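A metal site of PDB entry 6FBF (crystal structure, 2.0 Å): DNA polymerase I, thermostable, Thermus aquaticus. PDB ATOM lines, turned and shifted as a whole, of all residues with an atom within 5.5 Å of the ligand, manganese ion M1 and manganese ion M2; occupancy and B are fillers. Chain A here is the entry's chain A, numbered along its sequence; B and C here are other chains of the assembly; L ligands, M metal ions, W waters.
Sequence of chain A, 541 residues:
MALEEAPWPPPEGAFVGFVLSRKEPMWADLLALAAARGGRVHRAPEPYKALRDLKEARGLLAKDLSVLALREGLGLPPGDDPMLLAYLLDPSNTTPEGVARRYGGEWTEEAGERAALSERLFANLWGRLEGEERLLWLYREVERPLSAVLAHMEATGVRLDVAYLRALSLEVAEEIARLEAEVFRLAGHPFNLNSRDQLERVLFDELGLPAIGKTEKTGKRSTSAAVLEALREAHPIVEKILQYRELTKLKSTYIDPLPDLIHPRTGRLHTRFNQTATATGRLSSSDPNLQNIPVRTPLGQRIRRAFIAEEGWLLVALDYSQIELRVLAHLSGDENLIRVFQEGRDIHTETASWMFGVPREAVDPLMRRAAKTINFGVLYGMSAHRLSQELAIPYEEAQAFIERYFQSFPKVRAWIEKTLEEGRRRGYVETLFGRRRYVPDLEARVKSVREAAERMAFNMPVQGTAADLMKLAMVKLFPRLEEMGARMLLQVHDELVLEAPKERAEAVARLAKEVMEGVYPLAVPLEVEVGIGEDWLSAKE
Ser 321 touches the ligand (CA to O7, 3.6 Å). CZ of Phe 376 touches O6 of the ligand (3.2 Å). CD2 of Tyr 380 touches N2 of the ligand, 3.5 Å away. Of the 25 residues printed, 17 come within 4 Å of the ligand. The nearest printed residue that does not touch the ligand is Thr 373 (4.3 Å).
Water W6 lies within hydrogen-bond range of the side-chain carboxylate (OE1) of Glu 495 (2.6 Å) and the backbone carbonyl oxygen (O) of Val 492 (3.2 Å). Water W2 lies within hydrogen-bond range of O of Asp 319 (3.1 Å) and O7 of the ligand (3.5 Å). Water W4 lies within hydrogen-bond range of NH2 of Arg 369, OP2 of DC 12 of chain B and O5 of the ligand. Water W1 bridges an oxygen (O10) of the ligand and the side-chain amino group (NZ) of Lys 372. Water W7 lies within hydrogen-bond range of the side-chain carboxylate of Glu 324 (2.8 Å), the side-chain amide nitrogen of Gln 463 (2.9 Å), the side-chain amide nitrogen of Asn 459 (2.9 Å) and a nitrogen (N3) of the ligand (3.4 Å). Water W5 lies within hydrogen-bond range of the guanidinium group of Arg 282 (2.8 Å), the side-chain carboxylate of Glu 324 (2.8 Å) and an oxygen (O11) of the ligand (3.4 Å).
Within 4 Å of manganese ion M1: Asp 319, Tyr 320 and Asp 494.
The guanidinium group (NH1) of Arg 368 lies within salt-bridge range of an oxygen (O10) of the ligand (2.4 Å). NZ of Lys 372 lies within salt-bridge range of O10 of the ligand, at 2.7 Å. O2 of DC 4 of chain C sits at hydrogen-bond distance from N2 of the ligand, 2.7 Å away. O3 of the ligand sits close to N of Ile 323. NH1 of Arg 369 sits at hydrogen-bond distance from O1 of the ligand (2.9 Å). O6 of the ligand sits at hydrogen-bond distance from NE2 of His 348. The guanidinium group (NH2) of Arg 282 is in hydrogen-bond range of an oxygen (O11) of the ligand (3.2 Å). A nitrogen (N2) of the ligand lies close to N3 of DG 5 of chain C (3.4 Å). O8 of the ligand sits at hydrogen-bond distance from N of Glu 324, 3.2 Å away. The backbone NH (N) of Gln 322 sits at hydrogen-bond distance from an oxygen (O7) of the ligand, 3.3 Å away.
O2 of DC 12 of chain B is in hydrogen-bond range of the guanidinium group (NH1) of Arg 282 (2.9 Å). O2 of DC 12 of chain B lies close to N2 of DG 5 of chain C. The guanidinium group (NH2) of Arg 368 is in salt-bridge range of the side-chain carboxylate (OD2) of Asp 346 (3.0 Å). NH1 of Arg 369 lies within hydrogen-bond range of OG1 of Thr 373 (3.3 Å). The backbone NH (N) of His 348 sits at hydrogen-bond distance from the side-chain carboxylate (OD1) of Asp 346. N2 of DG 5 of chain C is in hydrogen-bond range of NH1 of Arg 282, 3.5 Å away. The side-chain amide oxygen of Gln 463 lies close to the guanidinium group of Arg 282 (3.5 Å). NE2 of Gln 322 is in hydrogen-bond range of OG of Ser 321 (3.4 Å).
OD1 of Asp 494 binds manganese ion M2, 2.1 Å away. OD2 of Asp 319 binds manganese ion M2 (2.2 Å). Water W6 binds manganese ion M2, 2.2 Å away. Manganese ion M2 is bound by water W3. An oxygen (O2) of the ligand is bound to manganese ion M2 (2.2 Å). O3' of DC 12 of chain B is bound to manganese ion M2.
Within 4 Å of manganese ion M2: Asp 319, Asp 494 and DC 12 of chain B. Along chain A the residues within 4 Å of manganese ion M2 span positions 319 to 494.
Manganese ion M1 is bound by an oxygen (O3) of the ligand, the backbone carbonyl oxygen (O) of Tyr 320, an oxygen (O4) of the ligand, the side-chain carboxylate (OD1) of Asp 319, the side-chain carboxylate (OD2) of Asp 494 and an oxygen (O2) of the ligand.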
ATOM      1  N   ARG A 282       8.896 -13.474  17.647  1.00  0.00           N
ATOM      2  CA  ARG A 282       8.306 -14.795  17.705  1.00  0.00           C
ATOM      3  C   ARG A 282       7.496 -14.976  18.988  1.00  0.00           C
ATOM      4  O   ARG A 282       7.764 -14.338  20.012  1.00  0.00           O
ATOM      5  CB  ARG A 282       9.393 -15.879  17.668  1.00  0.00           C
ATOM      6  CG  ARG A 282       9.821 -16.327  16.286  1.00  0.00           C
ATOM      7  CD  ARG A 282      10.722 -17.554  16.422  1.00  0.00           C
ATOM      8  NE  ARG A 282      11.048 -18.173  15.148  1.00  0.00           N
ATOM      9  CZ  ARG A 282      11.702 -19.320  15.024  1.00  0.00           C
ATOM     10  NH1 ARG A 282      12.082 -19.989  16.098  1.00  0.00           N
ATOM     11  NH2 ARG A 282      11.958 -19.805  13.814  1.00  0.00           N
ATOM     12  N   ASP A 319       2.225 -25.591   6.990  1.00  0.00           N
ATOM     13  CA  ASP A 319       3.582 -25.171   7.299  1.00  0.00           C
ATOM     14  C   ASP A 319       4.175 -24.455   6.095  1.00  0.00           C
ATOM     15  O   ASP A 319       4.207 -25.010   4.994  1.00  0.00           O
ATOM     16  CB  ASP A 319       4.448 -26.372   7.686  1.00  0.00           C
ATOM     17  CG  ASP A 319       5.838 -25.966   8.160  1.00  0.00           C
ATOM     18  OD1 ASP A 319       6.571 -25.318   7.379  1.00  0.00           O
ATOM     19  OD2 ASP A 319       6.203 -26.300   9.305  1.00  0.00           O
ATOM     20  N   TYR A 320       4.636 -23.220   6.295  1.00  0.00           N
ATOM     21  CA  TYR A 320       5.254 -22.461   5.214  1.00  0.00           C
ATOM     22  C   TYR A 320       6.498 -23.172   4.712  1.00  0.00           C
ATOM     23  O   TYR A 320       7.279 -23.741   5.494  1.00  0.00           O
ATOM     24  CB  TYR A 320       5.620 -21.052   5.691  1.00  0.00           C
ATOM     25  CG  TYR A 320       4.451 -20.102   5.825  1.00  0.00           C
ATOM     26  CD1 TYR A 320       3.899 -19.497   4.700  1.00  0.00           C
ATOM     27  CD2 TYR A 320       3.917 -19.789   7.067  1.00  0.00           C
ATOM     28  CE1 TYR A 320       2.841 -18.620   4.815  1.00  0.00           C
ATOM     29  CE2 TYR A 320       2.859 -18.913   7.182  1.00  0.00           C
ATOM     30  CZ  TYR A 320       2.326 -18.329   6.059  1.00  0.00           C
ATOM     31  OH  TYR A 320       1.268 -17.452   6.174  1.00  0.00           O
ATOM     32  N   SER A 321       6.693 -23.138   3.406  1.00  0.00           N
ATOM     33  CA  SER A 321       7.855 -23.752   2.769  1.00  0.00           C
ATOM     34  C   SER A 321       9.021 -22.756   2.773  1.00  0.00           C
ATOM     35  O   SER A 321       8.874 -21.630   2.271  1.00  0.00           O
ATOM     36  CB  SER A 321       7.530 -24.188   1.343  1.00  0.00           C
ATOM     37  OG  SER A 321       8.662 -24.725   0.696  1.00  0.00           O
ATOM     38  N   GLN A 322      10.160 -23.172   3.320  1.00  0.00           N
ATOM     39  CA  GLN A 322      11.403 -22.408   3.240  1.00  0.00           C
ATOM     40  C   GLN A 322      11.188 -20.950   3.620  1.00  0.00           C
ATOM     41  O   GLN A 322      11.644 -20.029   2.933  1.00  0.00           O
ATOM     42  CB  GLN A 322      12.012 -22.524   1.839  1.00  0.00           C
ATOM     43  CG  GLN A 322      12.112 -23.945   1.308  1.00  0.00           C
ATOM     44  CD  GLN A 322      12.552 -23.988  -0.140  1.00  0.00           C
ATOM     45  OE1 GLN A 322      13.721 -23.778  -0.464  1.00  0.00           O
ATOM     46  NE2 GLN A 322      11.604 -24.257  -1.036  1.00  0.00           N
ATOM     47  N   ILE A 323      10.492 -20.736   4.732  1.00  0.00           N
ATOM     48  CA  ILE A 323       9.915 -19.413   4.997  1.00  0.00           C
ATOM     49  C   ILE A 323      10.996 -18.337   5.036  1.00  0.00           C
ATOM     50  O   ILE A 323      10.925 -17.342   4.311  1.00  0.00           O
ATOM     51  CB  ILE A 323       9.066 -19.438   6.284  1.00  0.00           C
ATOM     52  CG1 ILE A 323       8.464 -18.059   6.570  1.00  0.00           C
ATOM     53  CG2 ILE A 323       9.859 -19.933   7.490  1.00  0.00           C
ATOM     54  CD1 ILE A 323       7.545 -17.545   5.473  1.00  0.00           C
ATOM     55  N   GLU A 324      12.018 -18.521   5.871  1.00  0.00           N
ATOM     56  CA  GLU A 324      12.993 -17.445   6.046  1.00  0.00           C
ATOM     57  C   GLU A 324      13.820 -17.219   4.787  1.00  0.00           C
ATOM     58  O   GLU A 324      14.265 -16.101   4.534  1.00  0.00           O
ATOM     59  CB  GLU A 324      13.902 -17.722   7.249  1.00  0.00           C
ATOM     60  CG  GLU A 324      13.237 -17.376   8.591  1.00  0.00           C
ATOM     61  CD  GLU A 324      14.216 -17.362   9.762  1.00  0.00           C
ATOM     62  OE1 GLU A 324      15.420 -17.103   9.545  1.00  0.00           O
ATOM     63  OE2 GLU A 324      13.775 -17.622  10.895  1.00  0.00           O
ATOM     64  N   LEU A 325      14.016 -18.261   3.975  1.00  0.00           N
ATOM     65  CA  LEU A 325      14.683 -18.076   2.692  1.00  0.00           C
ATOM     66  C   LEU A 325      13.834 -17.228   1.744  1.00  0.00           C
ATOM     67  O   LEU A 325      14.356 -16.364   1.044  1.00  0.00           O
ATOM     68  CB  LEU A 325      15.017 -19.428   2.057  1.00  0.00           C
ATOM     69  CG  LEU A 325      15.949 -20.346   2.855  1.00  0.00           C
ATOM     70  CD1 LEU A 325      16.306 -21.578   2.030  1.00  0.00           C
ATOM     71  CD2 LEU A 325      17.211 -19.619   3.303  1.00  0.00           C
ATOM     72  N   ASP A 346      13.643 -26.176  -4.391  1.00  0.00           N
ATOM     73  CA  ASP A 346      13.686 -26.395  -2.951  1.00  0.00           C
ATOM     74  C   ASP A 346      15.148 -26.471  -2.516  1.00  0.00           C
ATOM     75  O   ASP A 346      15.821 -27.467  -2.763  1.00  0.00           O
ATOM     76  CB  ASP A 346      12.931 -27.667  -2.569  1.00  0.00           C
ATOM     77  CG  ASP A 346      12.697 -27.798  -1.083  1.00  0.00           C
ATOM     78  OD1 ASP A 346      13.630 -27.542  -0.304  1.00  0.00           O
ATOM     79  OD2 ASP A 346      11.566 -28.158  -0.689  1.00  0.00           O
ATOM     80  N   HIS A 348      16.429 -26.680   0.472  1.00  0.00           N
ATOM     81  CA  HIS A 348      16.669 -27.710   1.469  1.00  0.00           C
ATOM     82  C   HIS A 348      16.899 -29.062   0.818  1.00  0.00           C
ATOM     83  O   HIS A 348      17.798 -29.805   1.204  1.00  0.00           O
ATOM     84  CB  HIS A 348      15.501 -27.770   2.453  1.00  0.00           C
ATOM     85  CG  HIS A 348      15.358 -26.534   3.294  1.00  0.00           C
ATOM     86  ND1 HIS A 348      16.386 -25.629   3.478  1.00  0.00           N
ATOM     87  CD2 HIS A 348      14.306 -26.055   3.995  1.00  0.00           C
ATOM     88  CE1 HIS A 348      15.964 -24.650   4.259  1.00  0.00           C
ATOM     89  NE2 HIS A 348      14.711 -24.887   4.589  1.00  0.00           N
ATOM     90  N   ARG A 368      16.577 -33.990   5.183  1.00  0.00           N
ATOM     91  CA  ARG A 368      16.191 -32.612   4.927  1.00  0.00           C
ATOM     92  C   ARG A 368      16.417 -31.737   6.149  1.00  0.00           C
ATOM     93  O   ARG A 368      16.872 -30.591   6.028  1.00  0.00           O
ATOM     94  CB  ARG A 368      14.730 -32.554   4.485  1.00  0.00           C
ATOM     95  CG  ARG A 368      14.335 -31.234   3.848  1.00  0.00           C
ATOM     96  CD  ARG A 368      13.199 -31.413   2.855  1.00  0.00           C
ATOM     97  NE  ARG A 368      12.820 -30.143   2.244  1.00  0.00           N
ATOM     98  CZ  ARG A 368      12.139 -29.199   2.881  1.00  0.00           C
ATOM     99  NH1 ARG A 368      11.772 -29.383   4.138  1.00  0.00           N
ATOM    100  NH2 ARG A 368      11.829 -28.069   2.252  1.00  0.00           N
ATOM    101  N   ARG A 369      16.119 -32.246   7.343  1.00  0.00           N
ATOM    102  CA  ARG A 369      16.401 -31.494   8.558  1.00  0.00           C
ATOM    103  C   ARG A 369      17.896 -31.202   8.676  1.00  0.00           C
ATOM    104  O   ARG A 369      18.294 -30.104   9.076  1.00  0.00           O
ATOM    105  CB  ARG A 369      15.900 -32.268   9.787  1.00  0.00           C
ATOM    106  CG  ARG A 369      16.238 -31.645  11.135  1.00  0.00           C
ATOM    107  CD  ARG A 369      15.671 -30.245  11.304  1.00  0.00           C
ATOM    108  NE  ARG A 369      16.685 -29.209  11.117  1.00  0.00           N
ATOM    109  CZ  ARG A 369      16.537 -27.931  11.475  1.00  0.00           C
ATOM    110  NH1 ARG A 369      17.519 -27.079  11.262  1.00  0.00           N
ATOM    111  NH2 ARG A 369      15.410 -27.520  12.030  1.00  0.00           N
ATOM    112  N   LYS A 372      18.654 -28.293   6.513  1.00  0.00           N
ATOM    113  CA  LYS A 372      18.221 -27.017   7.081  1.00  0.00           C
ATOM    114  C   LYS A 372      19.304 -26.407   7.961  1.00  0.00           C
ATOM    115  O   LYS A 372      19.595 -25.216   7.870  1.00  0.00           O
ATOM    116  CB  LYS A 372      16.928 -27.205   7.870  1.00  0.00           C
ATOM    117  CG  LYS A 372      15.720 -27.544   7.017  1.00  0.00           C
ATOM    118  CD  LYS A 372      14.497 -27.759   7.891  1.00  0.00           C
ATOM    119  CE  LYS A 372      13.246 -27.953   7.047  1.00  0.00           C
ATOM    120  NZ  LYS A 372      12.040 -28.165   7.883  1.00  0.00           N
ATOM    121  N   THR A 373      19.891 -27.220   8.837  1.00  0.00           N
ATOM    122  CA  THR A 373      20.975 -26.736   9.682  1.00  0.00           C
ATOM    123  C   THR A 373      22.056 -26.064   8.849  1.00  0.00           C
ATOM    124  O   THR A 373      22.534 -24.975   9.192  1.00  0.00           O
ATOM    125  CB  THR A 373      21.574 -27.887  10.496  1.00  0.00           C
ATOM    126  OG1 THR A 373      20.534 -28.506  11.276  1.00  0.00           O
ATOM    127  CG2 THR A 373      22.671 -27.393  11.435  1.00  0.00           C
ATOM    128  N   PHE A 376      20.638 -22.653   6.877  1.00  0.00           N
ATOM    129  CA  PHE A 376      20.492 -21.546   7.810  1.00  0.00           C
ATOM    130  C   PHE A 376      21.758 -21.303   8.609  1.00  0.00           C
ATOM    131  O   PHE A 376      22.077 -20.159   8.927  1.00  0.00           O
ATOM    132  CB  PHE A 376      19.294 -21.810   8.737  1.00  0.00           C
ATOM    133  CG  PHE A 376      17.976 -21.893   8.019  1.00  0.00           C
ATOM    134  CD1 PHE A 376      17.448 -20.779   7.379  1.00  0.00           C
ATOM    135  CD2 PHE A 376      17.272 -23.087   7.972  1.00  0.00           C
ATOM    136  CE1 PHE A 376      16.233 -20.852   6.705  1.00  0.00           C
ATOM    137  CE2 PHE A 376      16.058 -23.159   7.298  1.00  0.00           C
ATOM    138  CZ  PHE A 376      15.538 -22.046   6.663  1.00  0.00           C
ATOM    139  N   GLY A 377      22.501 -22.362   8.940  1.00  0.00           N
ATOM    140  CA  GLY A 377      23.768 -22.174   9.625  1.00  0.00           C
ATOM    141  C   GLY A 377      24.720 -21.310   8.834  1.00  0.00           C
ATOM    142  O   GLY A 377      25.272 -20.331   9.349  1.00  0.00           O
ATOM    143  N   TYR A 380      23.438 -17.520   8.513  1.00  0.00           N
ATOM    144  CA  TYR A 380      23.559 -16.695   9.710  1.00  0.00           C
ATOM    145  C   TYR A 380      24.943 -16.787  10.360  1.00  0.00           C
ATOM    146  O   TYR A 380      25.063 -16.582  11.572  1.00  0.00           O
ATOM    147  CB  TYR A 380      22.460 -17.064  10.707  1.00  0.00           C
ATOM    148  CG  TYR A 380      21.072 -16.777  10.163  1.00  0.00           C
ATOM    149  CD1 TYR A 380      20.690 -15.486   9.853  1.00  0.00           C
ATOM    150  CD2 TYR A 380      20.167 -17.803   9.948  1.00  0.00           C
ATOM    151  CE1 TYR A 380      19.437 -15.207   9.351  1.00  0.00           C
ATOM    152  CE2 TYR A 380      18.901 -17.545   9.443  1.00  0.00           C
ATOM    153  CZ  TYR A 380      18.537 -16.247   9.144  1.00  0.00           C
ATOM    154  OH  TYR A 380      17.284 -15.968   8.642  1.00  0.00           O
ATOM    155  N   ASN A 459      19.929 -11.383  11.754  1.00  0.00           N
ATOM    156  CA  ASN A 459      18.979 -12.487  11.782  1.00  0.00           C
ATOM    157  C   ASN A 459      17.580 -12.013  12.153  1.00  0.00           C
ATOM    158  O   ASN A 459      16.591 -12.556  11.640  1.00  0.00           O
ATOM    159  CB  ASN A 459      19.428 -13.559  12.775  1.00  0.00           C
ATOM    160  CG  ASN A 459      18.322 -14.539  13.125  1.00  0.00           C
ATOM    161  OD1 ASN A 459      17.506 -14.281  14.004  1.00  0.00           O
ATOM    162  ND2 ASN A 459      18.282 -15.672  12.420  1.00  0.00           N
ATOM    163  N   GLN A 463      13.971 -13.613  10.716  1.00  0.00           N
ATOM    164  CA  GLN A 463      13.100 -14.377  11.597  1.00  0.00           C
ATOM    165  C   GLN A 463      11.909 -13.545  12.064  1.00  0.00           C
ATOM    166  O   GLN A 463      10.802 -14.074  12.218  1.00  0.00           O
ATOM    167  CB  GLN A 463      13.904 -14.882  12.803  1.00  0.00           C
ATOM    168  CG  GLN A 463      13.110 -15.731  13.785  1.00  0.00           C
ATOM    169  CD  GLN A 463      13.926 -16.148  14.984  1.00  0.00           C
ATOM    170  OE1 GLN A 463      13.522 -15.945  16.132  1.00  0.00           O
ATOM    171  NE2 GLN A 463      15.091 -16.749  14.731  1.00  0.00           N
ATOM    172  N   VAL A 492       3.469 -23.186  15.533  1.00  0.00           N
ATOM    173  CA  VAL A 492       4.880 -23.540  15.697  1.00  0.00           C
ATOM    174  C   VAL A 492       5.712 -22.641  14.789  1.00  0.00           C
ATOM    175  O   VAL A 492       6.401 -23.121  13.892  1.00  0.00           O
ATOM    176  CB  VAL A 492       5.120 -25.027  15.401  1.00  0.00           C
ATOM    177  CG1 VAL A 492       6.418 -25.483  16.049  1.00  0.00           C
ATOM    178  CG2 VAL A 492       3.955 -25.878  15.889  1.00  0.00           C
ATOM    179  N   ASP A 494       6.099 -21.124  12.069  1.00  0.00           N
ATOM    180  CA  ASP A 494       5.644 -20.996  10.684  1.00  0.00           C
ATOM    181  C   ASP A 494       4.610 -22.071  10.350  1.00  0.00           C
ATOM    182  O   ASP A 494       4.382 -22.353   9.161  1.00  0.00           O
ATOM    183  CB  ASP A 494       6.823 -21.068   9.715  1.00  0.00           C
ATOM    184  CG  ASP A 494       7.319 -22.480   9.482  1.00  0.00           C
ATOM    185  OD1 ASP A 494       7.178 -23.328  10.392  1.00  0.00           O
ATOM    186  OD2 ASP A 494       7.860 -22.737   8.383  1.00  0.00           O
ATOM    187  N   GLU A 495       3.978 -22.648  11.362  1.00  0.00           N
ATOM    188  CA  GLU A 495       3.068 -23.771  11.179  1.00  0.00           C
ATOM    189  C   GLU A 495       1.832 -23.558  12.042  1.00  0.00           C
ATOM    190  O   GLU A 495       1.905 -22.958  13.119  1.00  0.00           O
ATOM    191  CB  GLU A 495       3.743 -25.099  11.540  1.00  0.00           C
ATOM    192  CG  GLU A 495       2.812 -26.321  11.546  1.00  0.00           C
ATOM    193  CD  GLU A 495       3.490 -27.565  12.093  1.00  0.00           C
ATOM    194  OE1 GLU A 495       4.680 -27.492  12.460  1.00  0.00           O
ATOM    195  OE2 GLU A 495       2.820 -28.624  12.150  1.00  0.00           O
ATOM    196  P    DC B  12      10.086 -29.003  13.894  1.00  0.00           P
ATOM    197  OP1  DC B  12       8.755 -29.332  13.361  1.00  0.00           O
ATOM    198  OP2  DC B  12      11.296 -29.574  13.262  1.00  0.00           O
ATOM    199  O5'  DC B  12      10.261 -27.421  13.915  1.00  0.00           O
ATOM    200  C5'  DC B  12       9.177 -26.592  14.342  1.00  0.00           C
ATOM    201  C4'  DC B  12       9.540 -25.124  14.260  1.00  0.00           C
ATOM    202  O4'  DC B  12      10.563 -24.838  15.237  1.00  0.00           O
ATOM    203  C3'  DC B  12      10.113 -24.674  12.935  1.00  0.00           C
ATOM    204  O3'  DC B  12       9.072 -24.291  12.047  1.00  0.00           O
ATOM    205  C2'  DC B  12      11.004 -23.504  13.315  1.00  0.00           C
ATOM    206  C1'  DC B  12      11.438 -23.829  14.745  1.00  0.00           C
ATOM    207  N1   DC B  12      12.836 -24.313  14.855  1.00  0.00           N
ATOM    208  C2   DC B  12      13.877 -23.400  14.989  1.00  0.00           C
ATOM    209  O2   DC B  12      13.608 -22.190  15.013  1.00  0.00           O
ATOM    210  N3   DC B  12      15.149 -23.856  15.092  1.00  0.00           N
ATOM    211  C4   DC B  12      15.386 -25.162  15.064  1.00  0.00           C
ATOM    212  N4   DC B  12      16.660 -25.577  15.172  1.00  0.00           N
ATOM    213  C5   DC B  12      14.339 -26.119  14.933  1.00  0.00           C
ATOM    214  C6   DC B  12      13.089 -25.653  14.833  1.00  0.00           C
ATOM    215  P    DC C   4      29.551 -21.245  14.904  1.00  0.00           P
ATOM    216  OP1  DC C   4      29.337 -22.333  15.887  1.00  0.00           O
ATOM    217  OP2  DC C   4      30.589 -21.392  13.860  1.00  0.00           O
ATOM    218  O5'  DC C   4      28.166 -20.942  14.167  1.00  0.00           O
ATOM    219  C5'  DC C   4      27.052 -20.494  14.920  1.00  0.00           C
ATOM    220  C4'  DC C   4      26.166 -19.595  14.091  1.00  0.00           C
ATOM    221  O4'  DC C   4      25.643 -20.338  12.970  1.00  0.00           O
ATOM    222  C3'  DC C   4      24.953 -19.038  14.823  1.00  0.00           C
ATOM    223  O3'  DC C   4      25.257 -17.806  15.462  1.00  0.00           O
ATOM    224  C2'  DC C   4      23.939 -18.879  13.699  1.00  0.00           C
ATOM    225  C1'  DC C   4      24.275 -20.034  12.773  1.00  0.00           C
ATOM    226  N1   DC C   4      23.467 -21.267  13.037  1.00  0.00           N
ATOM    227  C2   DC C   4      22.108 -21.272  12.694  1.00  0.00           C
ATOM    228  O2   DC C   4      21.609 -20.275  12.179  1.00  0.00           O
ATOM    229  N3   DC C   4      21.390 -22.398  12.936  1.00  0.00           N
ATOM    230  C4   DC C   4      21.960 -23.462  13.497  1.00  0.00           C
ATOM    231  N4   DC C   4      21.194 -24.538  13.711  1.00  0.00           N
ATOM    232  C5   DC C   4      23.346 -23.470  13.850  1.00  0.00           C
ATOM    233  C6   DC C   4      24.052 -22.355  13.608  1.00  0.00           C
ATOM    234  P    DG C   5      24.734 -17.519  16.959  1.00  0.00           P
ATOM    235  OP1  DG C   5      25.470 -16.347  17.462  1.00  0.00           O
ATOM    236  OP2  DG C   5      24.775 -18.798  17.704  1.00  0.00           O
ATOM    237  O5'  DG C   5      23.205 -17.123  16.751  1.00  0.00           O
ATOM    238  C5'  DG C   5      22.870 -15.945  16.045  1.00  0.00           C
ATOM    239  C4'  DG C   5      21.388 -15.897  15.718  1.00  0.00           C
ATOM    240  O4'  DG C   5      21.058 -16.983  14.813  1.00  0.00           O
ATOM    241  C3'  DG C   5      20.466 -16.092  16.904  1.00  0.00           C
ATOM    242  O3'  DG C   5      20.255 -14.871  17.599  1.00  0.00           O
ATOM    243  C2'  DG C   5      19.205 -16.615  16.239  1.00  0.00           C
ATOM    244  C1'  DG C   5      19.743 -17.444  15.077  1.00  0.00           C
ATOM    245  N9   DG C   5      19.782 -18.876  15.350  1.00  0.00           N
ATOM    246  C8   DG C   5      20.887 -19.628  15.671  1.00  0.00           C
ATOM    247  N7   DG C   5      20.608 -20.886  15.862  1.00  0.00           N
ATOM    248  C5   DG C   5      19.245 -20.970  15.652  1.00  0.00           C
ATOM    249  C6   DG C   5      18.372 -22.086  15.726  1.00  0.00           C
ATOM    250  O6   DG C   5      18.650 -23.266  15.978  1.00  0.00           O
ATOM    251  N1   DG C   5      17.050 -21.728  15.443  1.00  0.00           N
ATOM    252  C2   DG C   5      16.629 -20.453  15.142  1.00  0.00           C
ATOM    253  N2   DG C   5      15.317 -20.302  14.905  1.00  0.00           N
ATOM    254  N3   DG C   5      17.433 -19.407  15.078  1.00  0.00           N
ATOM    255  C4   DG C   5      18.722 -19.739  15.343  1.00  0.00           C
HETATM  256  N1  LIG L   1      18.678 -22.432  12.350  1.00  0.00           N
HETATM  257  C1  LIG L   1      18.125 -21.204  12.107  1.00  0.00           C
HETATM  258  N2  LIG L   1      18.934 -20.152  12.177  1.00  0.00           N
HETATM  259  N3  LIG L   1      16.829 -21.023  11.818  1.00  0.00           N
HETATM  260  C2  LIG L   1      16.137 -22.175  11.804  1.00  0.00           C
HETATM  261  C3  LIG L   1      16.598 -23.448  12.043  1.00  0.00           C
HETATM  262  C4  LIG L   1      17.992 -23.626  12.336  1.00  0.00           C
HETATM  263  O1  LIG L   1      18.573 -24.689  12.536  1.00  0.00           O
HETATM  264  N4  LIG L   1      15.553 -24.362  11.941  1.00  0.00           N
HETATM  265  C5  LIG L   1      14.509 -23.632  11.631  1.00  0.00           C
HETATM  266  N5  LIG L   1      14.802 -22.296  11.524  1.00  0.00           N
HETATM  267  P1  LIG L   1      10.942 -25.133   9.378  1.00  0.00           P
HETATM  268  P2  LIG L   1      11.469 -24.297   6.591  1.00  0.00           P
HETATM  269  P3  LIG L   1      10.210 -26.460   5.098  1.00  0.00           P
HETATM  270  C6  LIG L   1      13.918 -21.212  11.072  1.00  0.00           C
HETATM  271  O2  LIG L   1       9.413 -24.949   9.019  1.00  0.00           O
HETATM  272  O3  LIG L   1      10.257 -23.486   6.663  1.00  0.00           O
HETATM  273  O4  LIG L   1       8.971 -26.009   5.884  1.00  0.00           O
HETATM  274  C7  LIG L   1      14.054 -20.912   9.577  1.00  0.00           C
HETATM  275  O5  LIG L   1      11.108 -26.421  10.040  1.00  0.00           O
HETATM  276  O6  LIG L   1      12.670 -23.356   6.215  1.00  0.00           O
HETATM  277  O7  LIG L   1      10.002 -26.460   3.624  1.00  0.00           O
HETATM  278  C8  LIG L   1      12.905 -21.693   8.965  1.00  0.00           C
HETATM  279  O8  LIG L   1      12.496 -21.101   7.741  1.00  0.00           O
HETATM  280  N6  LIG L   1      11.810 -25.042   7.995  1.00  0.00           N
HETATM  281  O9  LIG L   1      11.372 -25.437   5.477  1.00  0.00           O
HETATM  282  O10 LIG L   1      10.655 -27.819   5.639  1.00  0.00           O
HETATM  283  C9  LIG L   1      11.837 -21.570  10.044  1.00  0.00           C
HETATM  284  O11 LIG L   1      12.564 -21.616  11.290  1.00  0.00           O
HETATM  285  C10 LIG L   1      10.768 -22.623  10.031  1.00  0.00           C
HETATM  286  O12 LIG L   1      11.365 -23.918  10.259  1.00  0.00           O
HETATM  287 MN    MN M   1       8.443 -24.346   7.092  1.00  0.00          MN
HETATM  288 MN    MN M   2       7.783 -25.382  10.457  1.00  0.00          MN
HETATM  289  O   HOH W   1       8.705 -28.167   7.939  1.00  0.00           O
HETATM  290  O   HOH W   2       6.676 -26.786   4.661  1.00  0.00           O
HETATM  291  O   HOH W   3       8.735 -27.352  10.752  1.00  0.00           O
HETATM  292  O   HOH W   4      12.953 -28.059  11.677  1.00  0.00           O
HETATM  293  O   HOH W   5      11.149 -18.498  11.476  1.00  0.00           O
HETATM  294  O   HOH W   6       6.631 -25.822  12.250  1.00  0.00           O
HETATM  295  O   HOH W   7      16.199 -17.729  12.265  1.00  0.00           O
